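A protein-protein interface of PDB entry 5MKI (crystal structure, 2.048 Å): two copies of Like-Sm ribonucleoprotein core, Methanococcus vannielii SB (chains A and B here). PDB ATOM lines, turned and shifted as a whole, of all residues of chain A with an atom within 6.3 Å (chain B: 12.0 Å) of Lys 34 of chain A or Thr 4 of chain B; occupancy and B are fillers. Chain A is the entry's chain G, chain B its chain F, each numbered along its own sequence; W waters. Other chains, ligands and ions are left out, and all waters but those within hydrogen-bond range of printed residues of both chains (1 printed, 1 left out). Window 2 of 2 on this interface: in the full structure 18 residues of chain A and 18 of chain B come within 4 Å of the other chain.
Water W1 lies within hydrogen-bond range of OXT of Leu 72 of chain B (2.5 Å) and O of Met 59 of chain A (2.9 Å).
The backbone carbonyl oxygen (O) of Ala 35 of chain A sits at hydrogen-bond distance from the backbone NH (N) of Ala 43 of chain A (2.8 Å).
NZ of Lys 34 of chain A lies within hydrogen-bond range of OD1 of Asn 16 of chain A (2.5 Å).
The side-chain carboxylate (OD1) of Asp 3 of chain B lies within hydrogen-bond range of the backbone NH (N) of Gln 5 of chain B, 2.7 Å away.
The backbone carbonyl oxygen (O) of Ala 43 of chain A lies within hydrogen-bond range of the backbone NH (N) of Lys 34 of chain A.
Among the printed residues, pairs that only touch across the chains: Ala 35 of chain A with Thr 4 of chain B, Tyr 36 of chain A with Pro 7 of chain B, Asp 37 of chain A with Pro 7 of chain B, Ala 35 of chain A with Pro 7 of chain B, Lys 34 of chain A with Thr 4 of chain B, Asp 37 of chain A with Gln 5 of chain B, Met 59 of chain A with Val 70 of chain B, Ala 35 of chain A with Asp 3 of chain B and Ala 43 of chain A with Pro 7 of chain B.
No residue of chain B comes within 4 Å of Asn 16 of chain A.
Arg 32 of chain A touches none of the printed residues of chain B.
Of chain B, only Asp 3 (3.8 Å), Thr 4 (3.3 Å) and Pro 7 (3.6 Å) come within 4 Å of Ala 35 of chain A.
Of chain B, only Pro 7 (3.8 Å) comes within 4 Å of Ala 43 of chain A.
No residue of chain B comes within 4 Å of Leu 44 of chain A.
No residue of chain B comes within 4 Å of Glu 45 of chain A.
Printed residues of chain A within 4 Å of Asp 3 of chain B: Ala 35.
Of the printed residues of chain A, Thr 4 of chain B touches Lys 34 (3.6 Å), Ala 35 (3.3 Å) and Tyr 36 (3.2 Å).
Printed residues of chain A within 4 Å of Val 70 of chain B: Met 59 (3.7 Å).
The nearest residue of chain B that does not touch Lys 34 of chain A is Asp 3 of chain B (4.8 Å).
No position is printed for both chains.
The backbone NH of Tyr 36 of chain A is in hydrogen-bond range of the backbone carbonyl oxygen of Thr 4 of chain B, at 3.2 Å.
The backbone carbonyl oxygen (O) of Tyr 36 of chain A lies close to the backbone carbonyl oxygen (O) of Gln 5 of chain B (3.2 Å).
The backbone NH of Leu 72 of chain B is in hydrogen-bond range of the backbone carbonyl oxygen of Met 59 of chain A (2.9 Å).
Of the 13 printed residues of chain A, 6 touch a printed residue of chain B.
Hydrophobic or aromatic side chains of chain A that line the printed part of chain B: Ala 35, Tyr 36 and Met 59.
Among the printed residues, 12 pairs touch across the chains.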
ATOM      1  N   ILE A  15      13.626   5.939 -35.532  1.00  0.00           N
ATOM      2  CA  ILE A  15      14.718   6.889 -35.387  1.00  0.00           C
ATOM      3  C   ILE A  15      14.713   7.884 -36.555  1.00  0.00           C
ATOM      4  O   ILE A  15      14.486   7.512 -37.715  1.00  0.00           O
ATOM      5  CB  ILE A  15      16.053   6.137 -35.276  1.00  0.00           C
ATOM      6  CG1 ILE A  15      16.261   5.679 -33.831  1.00  0.00           C
ATOM      7  CG2 ILE A  15      17.223   7.033 -35.682  1.00  0.00           C
ATOM      8  CD1 ILE A  15      16.569   6.835 -32.903  1.00  0.00           C
ATOM      9  N   ASN A  16      14.941   9.163 -36.233  1.00  0.00           N
ATOM     10  CA  ASN A  16      14.974  10.296 -37.162  1.00  0.00           C
ATOM     11  C   ASN A  16      13.619  10.595 -37.797  1.00  0.00           C
ATOM     12  O   ASN A  16      13.555  11.311 -38.798  1.00  0.00           O
ATOM     13  CB  ASN A  16      16.024  10.109 -38.262  1.00  0.00           C
ATOM     14  CG  ASN A  16      17.434  10.181 -37.728  1.00  0.00           C
ATOM     15  OD1 ASN A  16      17.725  10.959 -36.817  1.00  0.00           O
ATOM     16  ND2 ASN A  16      18.322   9.366 -38.287  1.00  0.00           N
ATOM     17  N   THR A  17      12.535  10.078 -37.231  1.00  0.00           N
ATOM     18  CA  THR A  17      11.187  10.511 -37.553  1.00  0.00           C
ATOM     19  C   THR A  17      10.612  11.282 -36.369  1.00  0.00           C
ATOM     20  O   THR A  17      11.153  11.259 -35.257  1.00  0.00           O
ATOM     21  CB  THR A  17      10.295   9.309 -37.886  1.00  0.00           C
ATOM     22  OG1 THR A  17       9.989   8.601 -36.675  1.00  0.00           O
ATOM     23  CG2 THR A  17      11.010   8.368 -38.854  1.00  0.00           C
ATOM     24  N   ARG A  32      11.759  15.206 -33.219  1.00  0.00           N
ATOM     25  CA  ARG A  32      12.386  14.138 -33.979  1.00  0.00           C
ATOM     26  C   ARG A  32      13.256  13.286 -33.065  1.00  0.00           C
ATOM     27  O   ARG A  32      14.157  13.801 -32.396  1.00  0.00           O
ATOM     28  CB  ARG A  32      13.217  14.681 -35.135  1.00  0.00           C
ATOM     29  CG  ARG A  32      13.888  13.561 -35.908  1.00  0.00           C
ATOM     30  CD  ARG A  32      14.598  14.093 -37.114  1.00  0.00           C
ATOM     31  NE  ARG A  32      13.674  14.831 -37.962  1.00  0.00           N
ATOM     32  CZ  ARG A  32      14.044  15.551 -39.009  1.00  0.00           C
ATOM     33  NH1 ARG A  32      15.332  15.634 -39.331  1.00  0.00           N
ATOM     34  NH2 ARG A  32      13.128  16.191 -39.720  1.00  0.00           N
ATOM     35  N   LEU A  33      13.008  11.980 -33.080  1.00  0.00           N
ATOM     36  CA  LEU A  33      13.691  11.031 -32.204  1.00  0.00           C
ATOM     37  C   LEU A  33      15.098  10.790 -32.720  1.00  0.00           C
ATOM     38  O   LEU A  33      15.284  10.221 -33.801  1.00  0.00           O
ATOM     39  CB  LEU A  33      12.914   9.719 -32.138  1.00  0.00           C
ATOM     40  CG  LEU A  33      13.560   8.660 -31.240  1.00  0.00           C
ATOM     41  CD1 LEU A  33      13.574   9.104 -29.759  1.00  0.00           C
ATOM     42  CD2 LEU A  33      12.819   7.340 -31.405  1.00  0.00           C
ATOM     43  N   LYS A  34      16.092  11.227 -31.949  1.00  0.00           N
ATOM     44  CA  LYS A  34      17.488  10.999 -32.290  1.00  0.00           C
ATOM     45  C   LYS A  34      18.095   9.812 -31.550  1.00  0.00           C
ATOM     46  O   LYS A  34      19.003   9.164 -32.088  1.00  0.00           O
ATOM     47  CB  LYS A  34      18.318  12.264 -32.009  1.00  0.00           C
ATOM     48  CG  LYS A  34      17.717  13.557 -32.581  1.00  0.00           C
ATOM     49  CD  LYS A  34      17.604  13.497 -34.111  1.00  0.00           C
ATOM     50  CE  LYS A  34      18.983  13.348 -34.734  1.00  0.00           C
ATOM     51  NZ  LYS A  34      18.938  13.113 -36.207  1.00  0.00           N
ATOM     52  N   ALA A  35      17.591   9.483 -30.356  1.00  0.00           N
ATOM     53  CA  ALA A  35      18.178   8.396 -29.578  1.00  0.00           C
ATOM     54  C   ALA A  35      17.216   7.966 -28.482  1.00  0.00           C
ATOM     55  O   ALA A  35      16.423   8.766 -27.976  1.00  0.00           O
ATOM     56  CB  ALA A  35      19.527   8.806 -28.958  1.00  0.00           C
ATOM     57  N   TYR A  36      17.305   6.689 -28.120  1.00  0.00           N
ATOM     58  CA  TYR A  36      16.569   6.153 -26.989  1.00  0.00           C
ATOM     59  C   TYR A  36      17.427   5.087 -26.326  1.00  0.00           C
ATOM     60  O   TYR A  36      18.383   4.583 -26.920  1.00  0.00           O
ATOM     61  CB  TYR A  36      15.226   5.557 -27.425  1.00  0.00           C
ATOM     62  CG  TYR A  36      15.399   4.286 -28.202  1.00  0.00           C
ATOM     63  CD1 TYR A  36      15.805   4.319 -29.533  1.00  0.00           C
ATOM     64  CD2 TYR A  36      15.160   3.051 -27.614  1.00  0.00           C
ATOM     65  CE1 TYR A  36      15.974   3.155 -30.257  1.00  0.00           C
ATOM     66  CE2 TYR A  36      15.331   1.881 -28.321  1.00  0.00           C
ATOM     67  CZ  TYR A  36      15.735   1.937 -29.648  1.00  0.00           C
ATOM     68  OH  TYR A  36      15.908   0.778 -30.371  1.00  0.00           O
ATOM     69  N   ASP A  37      17.071   4.727 -25.094  1.00  0.00           N
ATOM     70  CA  ASP A  37      17.708   3.567 -24.473  1.00  0.00           C
ATOM     71  C   ASP A  37      16.658   2.702 -23.780  1.00  0.00           C
ATOM     72  O   ASP A  37      15.459   2.996 -23.802  1.00  0.00           O
ATOM     73  CB  ASP A  37      18.787   4.001 -23.488  1.00  0.00           C
ATOM     74  CG  ASP A  37      18.237   4.850 -22.378  1.00  0.00           C
ATOM     75  OD1 ASP A  37      17.013   4.786 -22.074  1.00  0.00           O
ATOM     76  OD2 ASP A  37      19.046   5.597 -21.813  1.00  0.00           O
ATOM     77  N   ALA A  43      16.176  11.247 -26.754  1.00  0.00           N
ATOM     78  CA  ALA A  43      16.682  12.532 -27.218  1.00  0.00           C
ATOM     79  C   ALA A  43      15.812  13.003 -28.381  1.00  0.00           C
ATOM     80  O   ALA A  43      15.750  12.338 -29.424  1.00  0.00           O
ATOM     81  CB  ALA A  43      18.149  12.440 -27.639  1.00  0.00           C
ATOM     82  N   LEU A  44      15.155  14.143 -28.193  1.00  0.00           N
ATOM     83  CA  LEU A  44      14.260  14.744 -29.176  1.00  0.00           C
ATOM     84  C   LEU A  44      14.874  16.040 -29.702  1.00  0.00           C
ATOM     85  O   LEU A  44      15.167  16.955 -28.924  1.00  0.00           O
ATOM     86  CB  LEU A  44      12.901  15.023 -28.550  1.00  0.00           C
ATOM     87  CG  LEU A  44      12.244  13.757 -28.012  1.00  0.00           C
ATOM     88  CD1 LEU A  44      11.007  14.149 -27.239  1.00  0.00           C
ATOM     89  CD2 LEU A  44      11.923  12.816 -29.175  1.00  0.00           C
ATOM     90  N   GLU A  45      15.061  16.107 -31.018  1.00  0.00           N
ATOM     91  CA  GLU A  45      15.568  17.291 -31.704  1.00  0.00           C
ATOM     92  C   GLU A  45      14.423  18.193 -32.158  1.00  0.00           C
ATOM     93  O   GLU A  45      13.411  17.717 -32.685  1.00  0.00           O
ATOM     94  CB  GLU A  45      16.407  16.855 -32.903  1.00  0.00           C
ATOM     95  CG  GLU A  45      17.065  17.956 -33.688  1.00  0.00           C
ATOM     96  CD  GLU A  45      17.776  17.397 -34.915  1.00  0.00           C
ATOM     97  OE1 GLU A  45      17.090  16.899 -35.849  1.00  0.00           O
ATOM     98  OE2 GLU A  45      19.022  17.454 -34.947  1.00  0.00           O
ATOM     99  N   MET A  59      17.273  20.716 -28.649  1.00  0.00           N
ATOM    100  CA  MET A  59      17.541  19.333 -28.261  1.00  0.00           C
ATOM    101  C   MET A  59      17.051  19.113 -26.837  1.00  0.00           C
ATOM    102  O   MET A  59      17.434  19.846 -25.922  1.00  0.00           O
ATOM    103  CB  MET A  59      19.031  18.996 -28.387  1.00  0.00           C
ATOM    104  CG  MET A  59      19.393  17.543 -28.068  1.00  0.00           C
ATOM    105  SD  MET A  59      18.759  16.305 -29.223  1.00  0.00           S
ATOM    106  CE  MET A  59      19.454  16.884 -30.767  1.00  0.00           C
ATOM    107  N   ASP B   3      25.411   8.146 -31.132  1.00  0.00           N
ATOM    108  CA  ASP B   3      24.785   6.846 -31.342  1.00  0.00           C
ATOM    109  C   ASP B   3      23.318   6.883 -30.923  1.00  0.00           C
ATOM    110  O   ASP B   3      22.957   7.520 -29.928  1.00  0.00           O
ATOM    111  CB  ASP B   3      25.525   5.748 -30.573  1.00  0.00           C
ATOM    112  CG  ASP B   3      24.809   4.411 -30.643  1.00  0.00           C
ATOM    113  OD1 ASP B   3      24.035   4.112 -29.713  1.00  0.00           O
ATOM    114  OD2 ASP B   3      25.004   3.670 -31.637  1.00  0.00           O
ATOM    115  N   THR B   4      22.489   6.169 -31.685  1.00  0.00           N
ATOM    116  CA  THR B   4      21.040   6.208 -31.560  1.00  0.00           C
ATOM    117  C   THR B   4      20.516   5.397 -30.382  1.00  0.00           C
ATOM    118  O   THR B   4      19.296   5.327 -30.190  1.00  0.00           O
ATOM    119  CB  THR B   4      20.406   5.703 -32.861  1.00  0.00           C
ATOM    120  OG1 THR B   4      20.753   4.329 -33.051  1.00  0.00           O
ATOM    121  CG2 THR B   4      20.937   6.489 -34.035  1.00  0.00           C
ATOM    122  N   GLN B   5      21.399   4.768 -29.609  1.00  0.00           N
ATOM    123  CA  GLN B   5      21.023   4.031 -28.412  1.00  0.00           C
ATOM    124  C   GLN B   5      21.569   4.680 -27.151  1.00  0.00           C
ATOM    125  O   GLN B   5      21.445   4.106 -26.068  1.00  0.00           O
ATOM    126  CB  GLN B   5      21.517   2.590 -28.511  1.00  0.00           C
ATOM    127  CG  GLN B   5      20.685   1.732 -29.450  1.00  0.00           C
ATOM    128  CD  GLN B   5      21.413   0.475 -29.883  1.00  0.00           C
ATOM    129  OE1 GLN B   5      22.601   0.299 -29.598  1.00  0.00           O
ATOM    130  NE2 GLN B   5      20.707  -0.405 -30.585  1.00  0.00           N
ATOM    131  N   ARG B   6      22.178   5.860 -27.271  1.00  0.00           N
ATOM    132  CA  ARG B   6      22.794   6.567 -26.153  1.00  0.00           C
ATOM    133  C   ARG B   6      22.275   7.999 -26.104  1.00  0.00           C
ATOM    134  O   ARG B   6      23.000   8.953 -26.414  1.00  0.00           O
ATOM    135  CB  ARG B   6      24.317   6.527 -26.275  1.00  0.00           C
ATOM    136  CG  ARG B   6      24.865   5.119 -26.432  1.00  0.00           C
ATOM    137  CD  ARG B   6      26.366   5.086 -26.647  1.00  0.00           C
ATOM    138  NE  ARG B   6      26.838   3.712 -26.806  1.00  0.00           N
ATOM    139  CZ  ARG B   6      27.814   3.330 -27.629  1.00  0.00           C
ATOM    140  NH1 ARG B   6      28.452   4.221 -28.387  1.00  0.00           N
ATOM    141  NH2 ARG B   6      28.153   2.047 -27.698  1.00  0.00           N
ATOM    142  N   PRO B   7      21.022   8.188 -25.694  1.00  0.00           N
ATOM    143  CA  PRO B   7      20.487   9.556 -25.600  1.00  0.00           C
ATOM    144  C   PRO B   7      21.286  10.476 -24.682  1.00  0.00           C
ATOM    145  O   PRO B   7      21.395  11.675 -24.978  1.00  0.00           O
ATOM    146  CB  PRO B   7      19.052   9.333 -25.096  1.00  0.00           C
ATOM    147  CG  PRO B   7      19.065   7.926 -24.469  1.00  0.00           C
ATOM    148  CD  PRO B   7      20.029   7.163 -25.315  1.00  0.00           C
ATOM    149  N   LEU B   8      21.863   9.967 -23.587  1.00  0.00           N
ATOM    150  CA  LEU B   8      22.569  10.854 -22.664  1.00  0.00           C
ATOM    151  C   LEU B   8      23.901  11.361 -23.220  1.00  0.00           C
ATOM    152  O   LEU B   8      24.464  12.300 -22.646  1.00  0.00           O
ATOM    153  CB  LEU B   8      22.797  10.154 -21.309  1.00  0.00           C
ATOM    154  CG  LEU B   8      21.545   9.594 -20.599  1.00  0.00           C
ATOM    155  CD1 LEU B   8      21.859   9.130 -19.166  1.00  0.00           C
ATOM    156  CD2 LEU B   8      20.405  10.607 -20.572  1.00  0.00           C
ATOM    157  N   ASP B   9      24.417  10.771 -24.304  1.00  0.00           N
ATOM    158  CA  ASP B   9      25.575  11.344 -24.995  1.00  0.00           C
ATOM    159  C   ASP B   9      25.317  12.778 -25.456  1.00  0.00           C
ATOM    160  O   ASP B   9      26.267  13.549 -25.619  1.00  0.00           O
ATOM    161  CB  ASP B   9      25.966  10.494 -26.209  1.00  0.00           C
ATOM    162  CG  ASP B   9      26.835   9.292 -25.858  1.00  0.00           C
ATOM    163  OD1 ASP B   9      26.855   8.840 -24.691  1.00  0.00           O
ATOM    164  OD2 ASP B   9      27.492   8.779 -26.783  1.00  0.00           O
ATOM    165  N   ALA B  10      24.056  13.150 -25.706  1.00  0.00           N
ATOM    166  CA  ALA B  10      23.759  14.549 -26.007  1.00  0.00           C
ATOM    167  C   ALA B  10      24.158  15.457 -24.850  1.00  0.00           C
ATOM    168  O   ALA B  10      24.669  16.564 -25.063  1.00  0.00           O
ATOM    169  CB  ALA B  10      22.277  14.731 -26.327  1.00  0.00           C
ATOM    170  N   LEU B  11      23.911  15.018 -23.615  1.00  0.00           N
ATOM    171  CA  LEU B  11      24.417  15.770 -22.470  1.00  0.00           C
ATOM    172  C   LEU B  11      25.923  15.972 -22.595  1.00  0.00           C
ATOM    173  O   LEU B  11      26.427  17.078 -22.391  1.00  0.00           O
ATOM    174  CB  LEU B  11      24.069  15.059 -21.161  1.00  0.00           C
ATOM    175  CG  LEU B  11      22.645  15.165 -20.599  1.00  0.00           C
ATOM    176  CD1 LEU B  11      22.574  14.729 -19.120  1.00  0.00           C
ATOM    177  CD2 LEU B  11      22.143  16.562 -20.716  1.00  0.00           C
ATOM    178  N   LYS B  13      27.612  16.380 -25.205  1.00  0.00           N
ATOM    179  CA  LYS B  13      27.941  17.422 -26.174  1.00  0.00           C
ATOM    180  C   LYS B  13      27.684  18.823 -25.641  1.00  0.00           C
ATOM    181  O   LYS B  13      28.054  19.794 -26.305  1.00  0.00           O
ATOM    182  CB  LYS B  13      27.154  17.233 -27.478  1.00  0.00           C
ATOM    183  CG  LYS B  13      27.163  15.819 -28.035  1.00  0.00           C
ATOM    184  CD  LYS B  13      28.566  15.392 -28.390  1.00  0.00           C
ATOM    185  CE  LYS B  13      28.703  15.181 -29.887  1.00  0.00           C
ATOM    186  NZ  LYS B  13      27.541  14.418 -30.423  1.00  0.00           N
ATOM    187  N   VAL B  70      15.898  17.755 -19.937  1.00  0.00           N
ATOM    188  CA  VAL B  70      16.968  18.743 -19.989  1.00  0.00           C
ATOM    189  C   VAL B  70      16.959  19.388 -21.369  1.00  0.00           C
ATOM    190  O   VAL B  70      17.015  18.688 -22.389  1.00  0.00           O
ATOM    191  CB  VAL B  70      18.340  18.112 -19.688  1.00  0.00           C
ATOM    192  CG1 VAL B  70      19.437  19.159 -19.799  1.00  0.00           C
ATOM    193  CG2 VAL B  70      18.343  17.491 -18.289  1.00  0.00           C
ATOM    194  N   LEU B  72      18.943  21.428 -24.030  1.00  0.00           N
ATOM    195  CA  LEU B  72      20.331  21.704 -24.371  1.00  0.00           C
ATOM    196  C   LEU B  72      20.420  22.900 -25.319  1.00  0.00           C
ATOM    197  O   LEU B  72      21.378  23.677 -25.280  1.00  0.00           O
ATOM    198  CB  LEU B  72      20.975  20.462 -24.992  1.00  0.00           C
ATOM    199  CG  LEU B  72      20.756  19.189 -24.164  1.00  0.00           C
ATOM    200  CD1 LEU B  72      21.353  17.989 -24.852  1.00  0.00           C
ATOM    201  CD2 LEU B  72      21.396  19.386 -22.791  1.00  0.00           C
ATOM    202  OXT LEU B  72      19.518  23.129 -26.127  1.00  0.00           O
HETATM  203  O   HOH W   1      17.075  22.726 -26.229  1.00  0.00           O
